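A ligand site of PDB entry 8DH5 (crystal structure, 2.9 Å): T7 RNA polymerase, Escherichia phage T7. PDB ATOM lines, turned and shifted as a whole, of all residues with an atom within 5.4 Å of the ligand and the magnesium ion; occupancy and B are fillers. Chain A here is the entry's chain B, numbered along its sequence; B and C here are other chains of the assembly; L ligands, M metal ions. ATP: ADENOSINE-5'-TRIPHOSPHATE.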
ATOM      1  N   ASP A 471      -7.384 -31.409 -30.302  1.00  0.00           N
ATOM      2  CA  ASP A 471      -8.636 -31.390 -31.056  1.00  0.00           C
ATOM      3  C   ASP A 471      -8.912 -30.062 -31.755  1.00  0.00           C
ATOM      4  O   ASP A 471      -9.888 -29.968 -32.496  1.00  0.00           O
ATOM      5  CB  ASP A 471      -9.819 -31.733 -30.137  1.00  0.00           C
ATOM      6  CG  ASP A 471      -9.682 -31.124 -28.756  1.00  0.00           C
ATOM      7  OD1 ASP A 471      -9.071 -30.045 -28.640  1.00  0.00           O
ATOM      8  OD2 ASP A 471     -10.210 -31.715 -27.784  1.00  0.00           O
ATOM      9  N   LYS A 472      -8.082 -29.051 -31.527  1.00  0.00           N
ATOM     10  CA  LYS A 472      -8.265 -27.745 -32.149  1.00  0.00           C
ATOM     11  C   LYS A 472      -7.543 -27.642 -33.488  1.00  0.00           C
ATOM     12  O   LYS A 472      -7.492 -26.563 -34.072  1.00  0.00           O
ATOM     13  CB  LYS A 472      -7.771 -26.639 -31.217  1.00  0.00           C
ATOM     14  CG  LYS A 472      -8.235 -26.816 -29.798  1.00  0.00           C
ATOM     15  CD  LYS A 472      -9.753 -26.852 -29.764  1.00  0.00           C
ATOM     16  CE  LYS A 472     -10.263 -26.460 -28.410  1.00  0.00           C
ATOM     17  NZ  LYS A 472     -11.723 -26.757 -28.254  1.00  0.00           N
ATOM     18  N   SER A 539     -19.083 -30.229 -31.556  1.00  0.00           N
ATOM     19  CA  SER A 539     -18.518 -29.033 -30.925  1.00  0.00           C
ATOM     20  C   SER A 539     -19.432 -28.392 -29.892  1.00  0.00           C
ATOM     21  O   SER A 539     -19.246 -28.589 -28.681  1.00  0.00           O
ATOM     22  CB  SER A 539     -18.162 -28.009 -32.013  1.00  0.00           C
ATOM     23  OG  SER A 539     -19.317 -27.637 -32.747  1.00  0.00           O
ATOM     24  N   ASP A 569     -12.831 -22.331 -33.605  1.00  0.00           N
ATOM     25  CA  ASP A 569     -12.936 -22.211 -32.156  1.00  0.00           C
ATOM     26  C   ASP A 569     -13.877 -21.045 -31.860  1.00  0.00           C
ATOM     27  O   ASP A 569     -13.504 -19.881 -32.006  1.00  0.00           O
ATOM     28  CB  ASP A 569     -11.566 -21.996 -31.535  1.00  0.00           C
ATOM     29  CG  ASP A 569     -11.610 -21.902 -30.025  1.00  0.00           C
ATOM     30  OD1 ASP A 569     -12.292 -22.724 -29.391  1.00  0.00           O
ATOM     31  OD2 ASP A 569     -10.960 -20.993 -29.474  1.00  0.00           O
ATOM     32  N   TYR A 571     -15.056 -19.912 -29.086  1.00  0.00           N
ATOM     33  CA  TYR A 571     -14.570 -19.028 -28.029  1.00  0.00           C
ATOM     34  C   TYR A 571     -13.506 -18.082 -28.562  1.00  0.00           C
ATOM     35  O   TYR A 571     -13.495 -16.899 -28.234  1.00  0.00           O
ATOM     36  CB  TYR A 571     -14.031 -19.846 -26.849  1.00  0.00           C
ATOM     37  CG  TYR A 571     -14.779 -21.124 -26.562  1.00  0.00           C
ATOM     38  CD1 TYR A 571     -16.169 -21.119 -26.377  1.00  0.00           C
ATOM     39  CD2 TYR A 571     -14.118 -22.333 -26.451  1.00  0.00           C
ATOM     40  CE1 TYR A 571     -16.850 -22.281 -26.107  1.00  0.00           C
ATOM     41  CE2 TYR A 571     -14.795 -23.508 -26.180  1.00  0.00           C
ATOM     42  CZ  TYR A 571     -16.163 -23.475 -26.008  1.00  0.00           C
ATOM     43  OH  TYR A 571     -16.843 -24.645 -25.744  1.00  0.00           O
ATOM     44  N   ARG A 627      -9.372 -16.934 -25.496  1.00  0.00           N
ATOM     45  CA  ARG A 627     -10.575 -17.762 -25.530  1.00  0.00           C
ATOM     46  C   ARG A 627     -11.034 -18.179 -24.138  1.00  0.00           C
ATOM     47  O   ARG A 627     -12.210 -18.502 -23.971  1.00  0.00           O
ATOM     48  CB  ARG A 627     -10.306 -19.003 -26.381  1.00  0.00           C
ATOM     49  CG  ARG A 627      -9.028 -19.728 -26.002  1.00  0.00           C
ATOM     50  CD  ARG A 627      -8.596 -20.713 -27.065  1.00  0.00           C
ATOM     51  NE  ARG A 627      -9.691 -21.600 -27.449  1.00  0.00           N
ATOM     52  CZ  ARG A 627     -10.102 -22.640 -26.733  1.00  0.00           C
ATOM     53  NH1 ARG A 627      -9.529 -22.965 -25.588  1.00  0.00           N
ATOM     54  NH2 ARG A 627     -11.121 -23.359 -27.178  1.00  0.00           N
ATOM     55  N   LYS A 631     -14.852 -18.315 -22.836  1.00  0.00           N
ATOM     56  CA  LYS A 631     -15.192 -19.723 -23.006  1.00  0.00           C
ATOM     57  C   LYS A 631     -16.519 -20.085 -22.347  1.00  0.00           C
ATOM     58  O   LYS A 631     -17.485 -20.416 -23.046  1.00  0.00           O
ATOM     59  CB  LYS A 631     -14.087 -20.621 -22.453  1.00  0.00           C
ATOM     60  CG  LYS A 631     -14.198 -22.083 -22.874  1.00  0.00           C
ATOM     61  CD  LYS A 631     -13.800 -23.018 -21.739  1.00  0.00           C
ATOM     62  CE  LYS A 631     -12.475 -23.693 -22.013  1.00  0.00           C
ATOM     63  NZ  LYS A 631     -12.385 -25.026 -21.362  1.00  0.00           N
ATOM     64  N   ARG A 632     -16.572 -19.989 -21.017  1.00  0.00           N
ATOM     65  CA  ARG A 632     -17.764 -20.388 -20.255  1.00  0.00           C
ATOM     66  C   ARG A 632     -18.995 -19.591 -20.664  1.00  0.00           C
ATOM     67  O   ARG A 632     -20.129 -20.086 -20.564  1.00  0.00           O
ATOM     68  CB  ARG A 632     -17.480 -20.236 -18.765  1.00  0.00           C
ATOM     69  CG  ARG A 632     -18.643 -20.571 -17.835  1.00  0.00           C
ATOM     70  CD  ARG A 632     -18.248 -21.491 -16.688  1.00  0.00           C
ATOM     71  NE  ARG A 632     -17.967 -22.859 -17.127  1.00  0.00           N
ATOM     72  CZ  ARG A 632     -18.892 -23.764 -17.408  1.00  0.00           C
ATOM     73  NH1 ARG A 632     -20.184 -23.467 -17.382  1.00  0.00           N
ATOM     74  NH2 ARG A 632     -18.524 -24.995 -17.711  1.00  0.00           N
ATOM     75  N   MET A 635     -20.501 -21.336 -23.721  1.00  0.00           N
ATOM     76  CA  MET A 635     -21.021 -22.658 -23.413  1.00  0.00           C
ATOM     77  C   MET A 635     -22.366 -22.589 -22.710  1.00  0.00           C
ATOM     78  O   MET A 635     -23.223 -23.465 -22.917  1.00  0.00           O
ATOM     79  CB  MET A 635     -20.021 -23.435 -22.568  1.00  0.00           C
ATOM     80  CG  MET A 635     -18.613 -23.387 -23.115  1.00  0.00           C
ATOM     81  SD  MET A 635     -17.402 -24.356 -22.185  1.00  0.00           S
ATOM     82  CE  MET A 635     -18.454 -25.208 -21.019  1.00  0.00           C
ATOM     83  N   TYR A 639     -27.976 -22.663 -22.467  1.00  0.00           N
ATOM     84  CA  TYR A 639     -28.706 -22.822 -21.220  1.00  0.00           C
ATOM     85  C   TYR A 639     -29.462 -21.550 -20.824  1.00  0.00           C
ATOM     86  O   TYR A 639     -30.234 -21.586 -19.861  1.00  0.00           O
ATOM     87  CB  TYR A 639     -27.760 -23.231 -20.088  1.00  0.00           C
ATOM     88  CG  TYR A 639     -27.002 -24.513 -20.360  1.00  0.00           C
ATOM     89  CD1 TYR A 639     -27.593 -25.560 -21.066  1.00  0.00           C
ATOM     90  CD2 TYR A 639     -25.701 -24.687 -19.915  1.00  0.00           C
ATOM     91  CE1 TYR A 639     -26.908 -26.729 -21.316  1.00  0.00           C
ATOM     92  CE2 TYR A 639     -25.006 -25.853 -20.166  1.00  0.00           C
ATOM     93  CZ  TYR A 639     -25.612 -26.882 -20.865  1.00  0.00           C
ATOM     94  OH  TYR A 639     -24.939 -28.048 -21.121  1.00  0.00           O
ATOM     95  N   ASP A 812     -23.748 -35.762 -26.550  1.00  0.00           N
ATOM     96  CA  ASP A 812     -22.978 -35.054 -27.568  1.00  0.00           C
ATOM     97  C   ASP A 812     -22.090 -35.981 -28.386  1.00  0.00           C
ATOM     98  O   ASP A 812     -21.856 -35.721 -29.571  1.00  0.00           O
ATOM     99  CB  ASP A 812     -22.108 -34.001 -26.890  1.00  0.00           C
ATOM    100  CG  ASP A 812     -22.833 -32.703 -26.710  1.00  0.00           C
ATOM    101  OD1 ASP A 812     -22.692 -31.841 -27.599  1.00  0.00           O
ATOM    102  OD2 ASP A 812     -23.580 -32.564 -25.717  1.00  0.00           O
ATOM    103  P     A B  11     -16.465 -34.961 -15.545  1.00  0.00           P
ATOM    104  OP1   A B  11     -15.339 -35.454 -16.365  1.00  0.00           O
ATOM    105  OP2   A B  11     -16.548 -33.522 -15.183  1.00  0.00           O
ATOM    106  O5'   A B  11     -17.822 -35.384 -16.276  1.00  0.00           O
ATOM    107  C5'   A B  11     -18.027 -36.713 -16.704  1.00  0.00           C
ATOM    108  C4'   A B  11     -19.381 -36.887 -17.340  1.00  0.00           C
ATOM    109  O4'   A B  11     -20.431 -36.697 -16.359  1.00  0.00           O
ATOM    110  C3'   A B  11     -19.727 -35.888 -18.431  1.00  0.00           C
ATOM    111  O3'   A B  11     -19.104 -36.172 -19.670  1.00  0.00           O
ATOM    112  C2'   A B  11     -21.255 -35.963 -18.463  1.00  0.00           C
ATOM    113  O2'   A B  11     -21.700 -37.125 -19.142  1.00  0.00           O
ATOM    114  C1'   A B  11     -21.563 -36.128 -16.979  1.00  0.00           C
ATOM    115  N9    A B  11     -21.861 -34.834 -16.327  1.00  0.00           N
ATOM    116  C8    A B  11     -21.069 -34.117 -15.465  1.00  0.00           C
ATOM    117  N7    A B  11     -21.609 -32.991 -15.054  1.00  0.00           N
ATOM    118  C5    A B  11     -22.833 -32.967 -15.697  1.00  0.00           C
ATOM    119  C6    A B  11     -23.898 -32.040 -15.691  1.00  0.00           C
ATOM    120  N6    A B  11     -23.880 -30.915 -14.976  1.00  0.00           N
ATOM    121  N1    A B  11     -24.986 -32.312 -16.440  1.00  0.00           N
ATOM    122  C2    A B  11     -25.002 -33.443 -17.148  1.00  0.00           C
ATOM    123  N3    A B  11     -24.070 -34.399 -17.242  1.00  0.00           N
ATOM    124  C4    A B  11     -23.002 -34.088 -16.481  1.00  0.00           C
ATOM    125  P     U B  12     -18.452 -34.978 -20.509  1.00  0.00           P
ATOM    126  OP1   U B  12     -17.615 -35.614 -21.547  1.00  0.00           O
ATOM    127  OP2   U B  12     -17.810 -34.060 -19.541  1.00  0.00           O
ATOM    128  O5'   U B  12     -19.704 -34.296 -21.195  1.00  0.00           O
ATOM    129  C5'   U B  12     -20.479 -35.085 -22.092  1.00  0.00           C
ATOM    130  C4'   U B  12     -21.836 -34.477 -22.330  1.00  0.00           C
ATOM    131  O4'   U B  12     -22.554 -34.325 -21.076  1.00  0.00           O
ATOM    132  C3'   U B  12     -21.830 -33.086 -22.936  1.00  0.00           C
ATOM    133  C2'   U B  12     -23.201 -32.569 -22.528  1.00  0.00           C
ATOM    134  O2'   U B  12     -24.184 -33.109 -23.390  1.00  0.00           O
ATOM    135  C1'   U B  12     -23.369 -33.175 -21.131  1.00  0.00           C
ATOM    136  N1    U B  12     -23.015 -32.179 -20.095  1.00  0.00           N
ATOM    137  C2    U B  12     -23.991 -31.280 -19.737  1.00  0.00           C
ATOM    138  O2    U B  12     -25.120 -31.278 -20.223  1.00  0.00           O
ATOM    139  N3    U B  12     -23.612 -30.373 -18.778  1.00  0.00           N
ATOM    140  C4    U B  12     -22.377 -30.277 -18.167  1.00  0.00           C
ATOM    141  O4    U B  12     -22.186 -29.403 -17.317  1.00  0.00           O
ATOM    142  C5    U B  12     -21.419 -31.256 -18.591  1.00  0.00           C
ATOM    143  C6    U B  12     -21.758 -32.139 -19.522  1.00  0.00           C
ATOM    144  C12 S8U C  10     -24.930 -22.332 -15.893  1.00  0.00           C
ATOM    145  C13 S8U C  10     -24.997 -23.849 -16.018  1.00  0.00           C
ATOM    146  C1' S8U C  10     -27.258 -21.784 -16.162  1.00  0.00           C
ATOM    147  C15 S8U C  10     -23.758 -21.577 -15.666  1.00  0.00           C
ATOM    148  C16 S8U C  10     -24.109 -20.261 -15.621  1.00  0.00           C
ATOM    149  C17 S8U C  10     -25.478 -20.173 -15.802  1.00  0.00           C
ATOM    150  C2' S8U C  10     -28.060 -21.556 -14.829  1.00  0.00           C
ATOM    151  C3' S8U C  10     -29.212 -21.416 -15.201  1.00  0.00           C
ATOM    152  C4' S8U C  10     -29.115 -20.654 -16.675  1.00  0.00           C
ATOM    153  C5' S8U C  10     -29.383 -19.185 -16.482  1.00  0.00           C
ATOM    154  N11 S8U C  10     -25.981 -21.462 -15.975  1.00  0.00           N
ATOM    155  O14 S8U C  10     -24.022 -24.463 -16.184  1.00  0.00           O
ATOM    156  O3' S8U C  10     -29.839 -22.762 -15.330  1.00  0.00           O
ATOM    157  O4' S8U C  10     -27.949 -20.839 -17.132  1.00  0.00           O
ATOM    158  O5' S8U C  10     -28.169 -18.503 -16.458  1.00  0.00           O
ATOM    159  OP1 S8U C  10     -27.595 -17.655 -14.041  1.00  0.00           O
ATOM    160  OP2 S8U C  10     -26.784 -16.442 -15.995  1.00  0.00           O
ATOM    161  P   S8U C  10     -27.900 -17.239 -15.447  1.00  0.00           P
ATOM    162  P    DA C  11     -31.428 -22.934 -15.463  1.00  0.00           P
ATOM    163  OP1  DA C  11     -32.046 -21.589 -15.317  1.00  0.00           O
ATOM    164  OP2  DA C  11     -31.835 -24.030 -14.567  1.00  0.00           O
ATOM    165  O5'  DA C  11     -31.618 -23.437 -16.967  1.00  0.00           O
ATOM    166  C5'  DA C  11     -32.821 -24.076 -17.358  1.00  0.00           C
ATOM    167  C4'  DA C  11     -32.525 -25.371 -18.089  1.00  0.00           C
ATOM    168  O4'  DA C  11     -31.252 -25.268 -18.777  1.00  0.00           O
ATOM    169  C3'  DA C  11     -32.359 -26.591 -17.211  1.00  0.00           C
ATOM    170  O3'  DA C  11     -33.618 -27.115 -16.833  1.00  0.00           O
ATOM    171  C2'  DA C  11     -31.626 -27.528 -18.159  1.00  0.00           C
ATOM    172  C1'  DA C  11     -30.670 -26.565 -18.860  1.00  0.00           C
ATOM    173  N9   DA C  11     -29.344 -26.522 -18.246  1.00  0.00           N
ATOM    174  C8   DA C  11     -28.823 -25.540 -17.444  1.00  0.00           C
ATOM    175  N7   DA C  11     -27.605 -25.774 -17.038  1.00  0.00           N
ATOM    176  C5   DA C  11     -27.302 -27.007 -17.606  1.00  0.00           C
ATOM    177  C6   DA C  11     -26.146 -27.816 -17.546  1.00  0.00           C
ATOM    178  N6   DA C  11     -25.044 -27.487 -16.864  1.00  0.00           N
ATOM    179  N1   DA C  11     -26.167 -28.984 -18.226  1.00  0.00           N
ATOM    180  C2   DA C  11     -27.269 -29.313 -18.908  1.00  0.00           C
ATOM    181  N3   DA C  11     -28.417 -28.634 -19.031  1.00  0.00           N
ATOM    182  C4   DA C  11     -28.357 -27.482 -18.339  1.00  0.00           C
HETATM  183  PG  ATP L   1     -11.730 -26.576 -24.942  1.00  0.00           P
HETATM  184  O1G ATP L   1     -11.224 -27.825 -25.590  1.00  0.00           O
HETATM  185  O2G ATP L   1     -11.240 -26.400 -23.502  1.00  0.00           O
HETATM  186  O3G ATP L   1     -11.455 -25.286 -25.704  1.00  0.00           O
HETATM  187  PB  ATP L   1     -14.457 -27.667 -24.494  1.00  0.00           P
HETATM  188  O1B ATP L   1     -15.733 -27.304 -25.147  1.00  0.00           O
HETATM  189  O2B ATP L   1     -13.916 -29.061 -24.818  1.00  0.00           O
HETATM  190  O3B ATP L   1     -13.312 -26.631 -24.819  1.00  0.00           O
HETATM  191  PA  ATP L   1     -14.016 -28.380 -21.655  1.00  0.00           P
HETATM  192  O1A ATP L   1     -12.562 -28.607 -21.732  1.00  0.00           O
HETATM  193  O2A ATP L   1     -14.863 -29.658 -21.579  1.00  0.00           O
HETATM  194  O3A ATP L   1     -14.548 -27.552 -22.909  1.00  0.00           O
HETATM  195  O5' ATP L   1     -14.397 -27.466 -20.417  1.00  0.00           O
HETATM  196  C5' ATP L   1     -14.299 -27.962 -19.068  1.00  0.00           C
HETATM  197  C4' ATP L   1     -15.387 -27.363 -18.209  1.00  0.00           C
HETATM  198  O4' ATP L   1     -16.613 -27.253 -18.957  1.00  0.00           O
HETATM  199  C3' ATP L   1     -15.739 -28.176 -16.963  1.00  0.00           C
HETATM  200  O3' ATP L   1     -16.176 -27.322 -15.918  1.00  0.00           O
HETATM  201  C2' ATP L   1     -16.875 -29.067 -17.478  1.00  0.00           C
HETATM  202  O2' ATP L   1     -17.720 -29.504 -16.409  1.00  0.00           O
HETATM  203  C1' ATP L   1     -17.611 -28.078 -18.384  1.00  0.00           C
HETATM  204  N9  ATP L   1     -18.390 -28.677 -19.465  1.00  0.00           N
HETATM  205  C8  ATP L   1     -18.027 -29.699 -20.306  1.00  0.00           C
HETATM  206  N7  ATP L   1     -18.939 -30.003 -21.202  1.00  0.00           N
HETATM  207  C5  ATP L   1     -19.976 -29.124 -20.927  1.00  0.00           C
HETATM  208  C6  ATP L   1     -21.245 -28.922 -21.509  1.00  0.00           C
HETATM  209  N6  ATP L   1     -21.705 -29.638 -22.542  1.00  0.00           N
HETATM  210  N1  ATP L   1     -22.034 -27.963 -20.995  1.00  0.00           N
HETATM  211  C2  ATP L   1     -21.588 -27.236 -19.963  1.00  0.00           C
HETATM  212  N3  ATP L   1     -20.416 -27.337 -19.331  1.00  0.00           N
HETATM  213  C4  ATP L   1     -19.652 -28.291 -19.857  1.00  0.00           C
HETATM  214 MG    MG M   1     -11.234 -29.979 -25.075  1.00  0.00          MG
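O3G of the ligand lies within salt-bridge range of NZ of Lys 472, 3.0 Å away. O2G of the ligand lies within salt-bridge range of NZ of Lys 631 (2.8 Å). An oxygen (O3G) of the ligand lies within salt-bridge range of the guanidinium group of Arg 627, at 2.4 Å. O1B of the ligand sits at hydrogen-bond distance from OH of Tyr 571 (2.9 Å). The side-chain hydroxyl (OH) of Tyr 639 sits at hydrogen-bond distance from a nitrogen (N1) of the ligand, at 2.9 Å. The guanidinium group (NH2) of Arg 632 lies within hydrogen-bond range of an oxygen (O4') of the ligand (3.2 Å).
O2' of U 12 of chain B lies close to the side-chain carboxylate of Asp 812 (2.5 Å). The side-chain hydroxyl (OH) of Tyr 639 lies within hydrogen-bond range of O2 of U 12 of chain B (3.4 Å). NE of Arg 627 lies within salt-bridge range of OD2 of Asp 569 (2.5 Å). The side-chain sulfur (SD) of Met 635 sits close to the side-chain hydroxyl (OH) of Tyr 571, 3.6 Å away. The side-chain hydroxyl of Tyr 639 lies within hydrogen-bond range of N1 of DA 11 of chain C, at 3.3 Å.
A nitrogen (N3) of the ligand lies close to O4 of U 12 of chain B. Met 635 touches the ligand (CE to N3, 3.4 Å). Along chain A the residues within 4 Å of the ligand span positions 472 to 639. The nearest printed residue that does not touch the ligand is Asp 471 (4.3 Å).
Asp 471 touches the magnesium ion (OD2 to MG, 3.4 Å).
The magnesium ion is bound by O1G of the ligand. The magnesium ion has one donor atom within binding distance. Slightly farther from the magnesium ion lies O2B of the ligand (2.8 Å).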
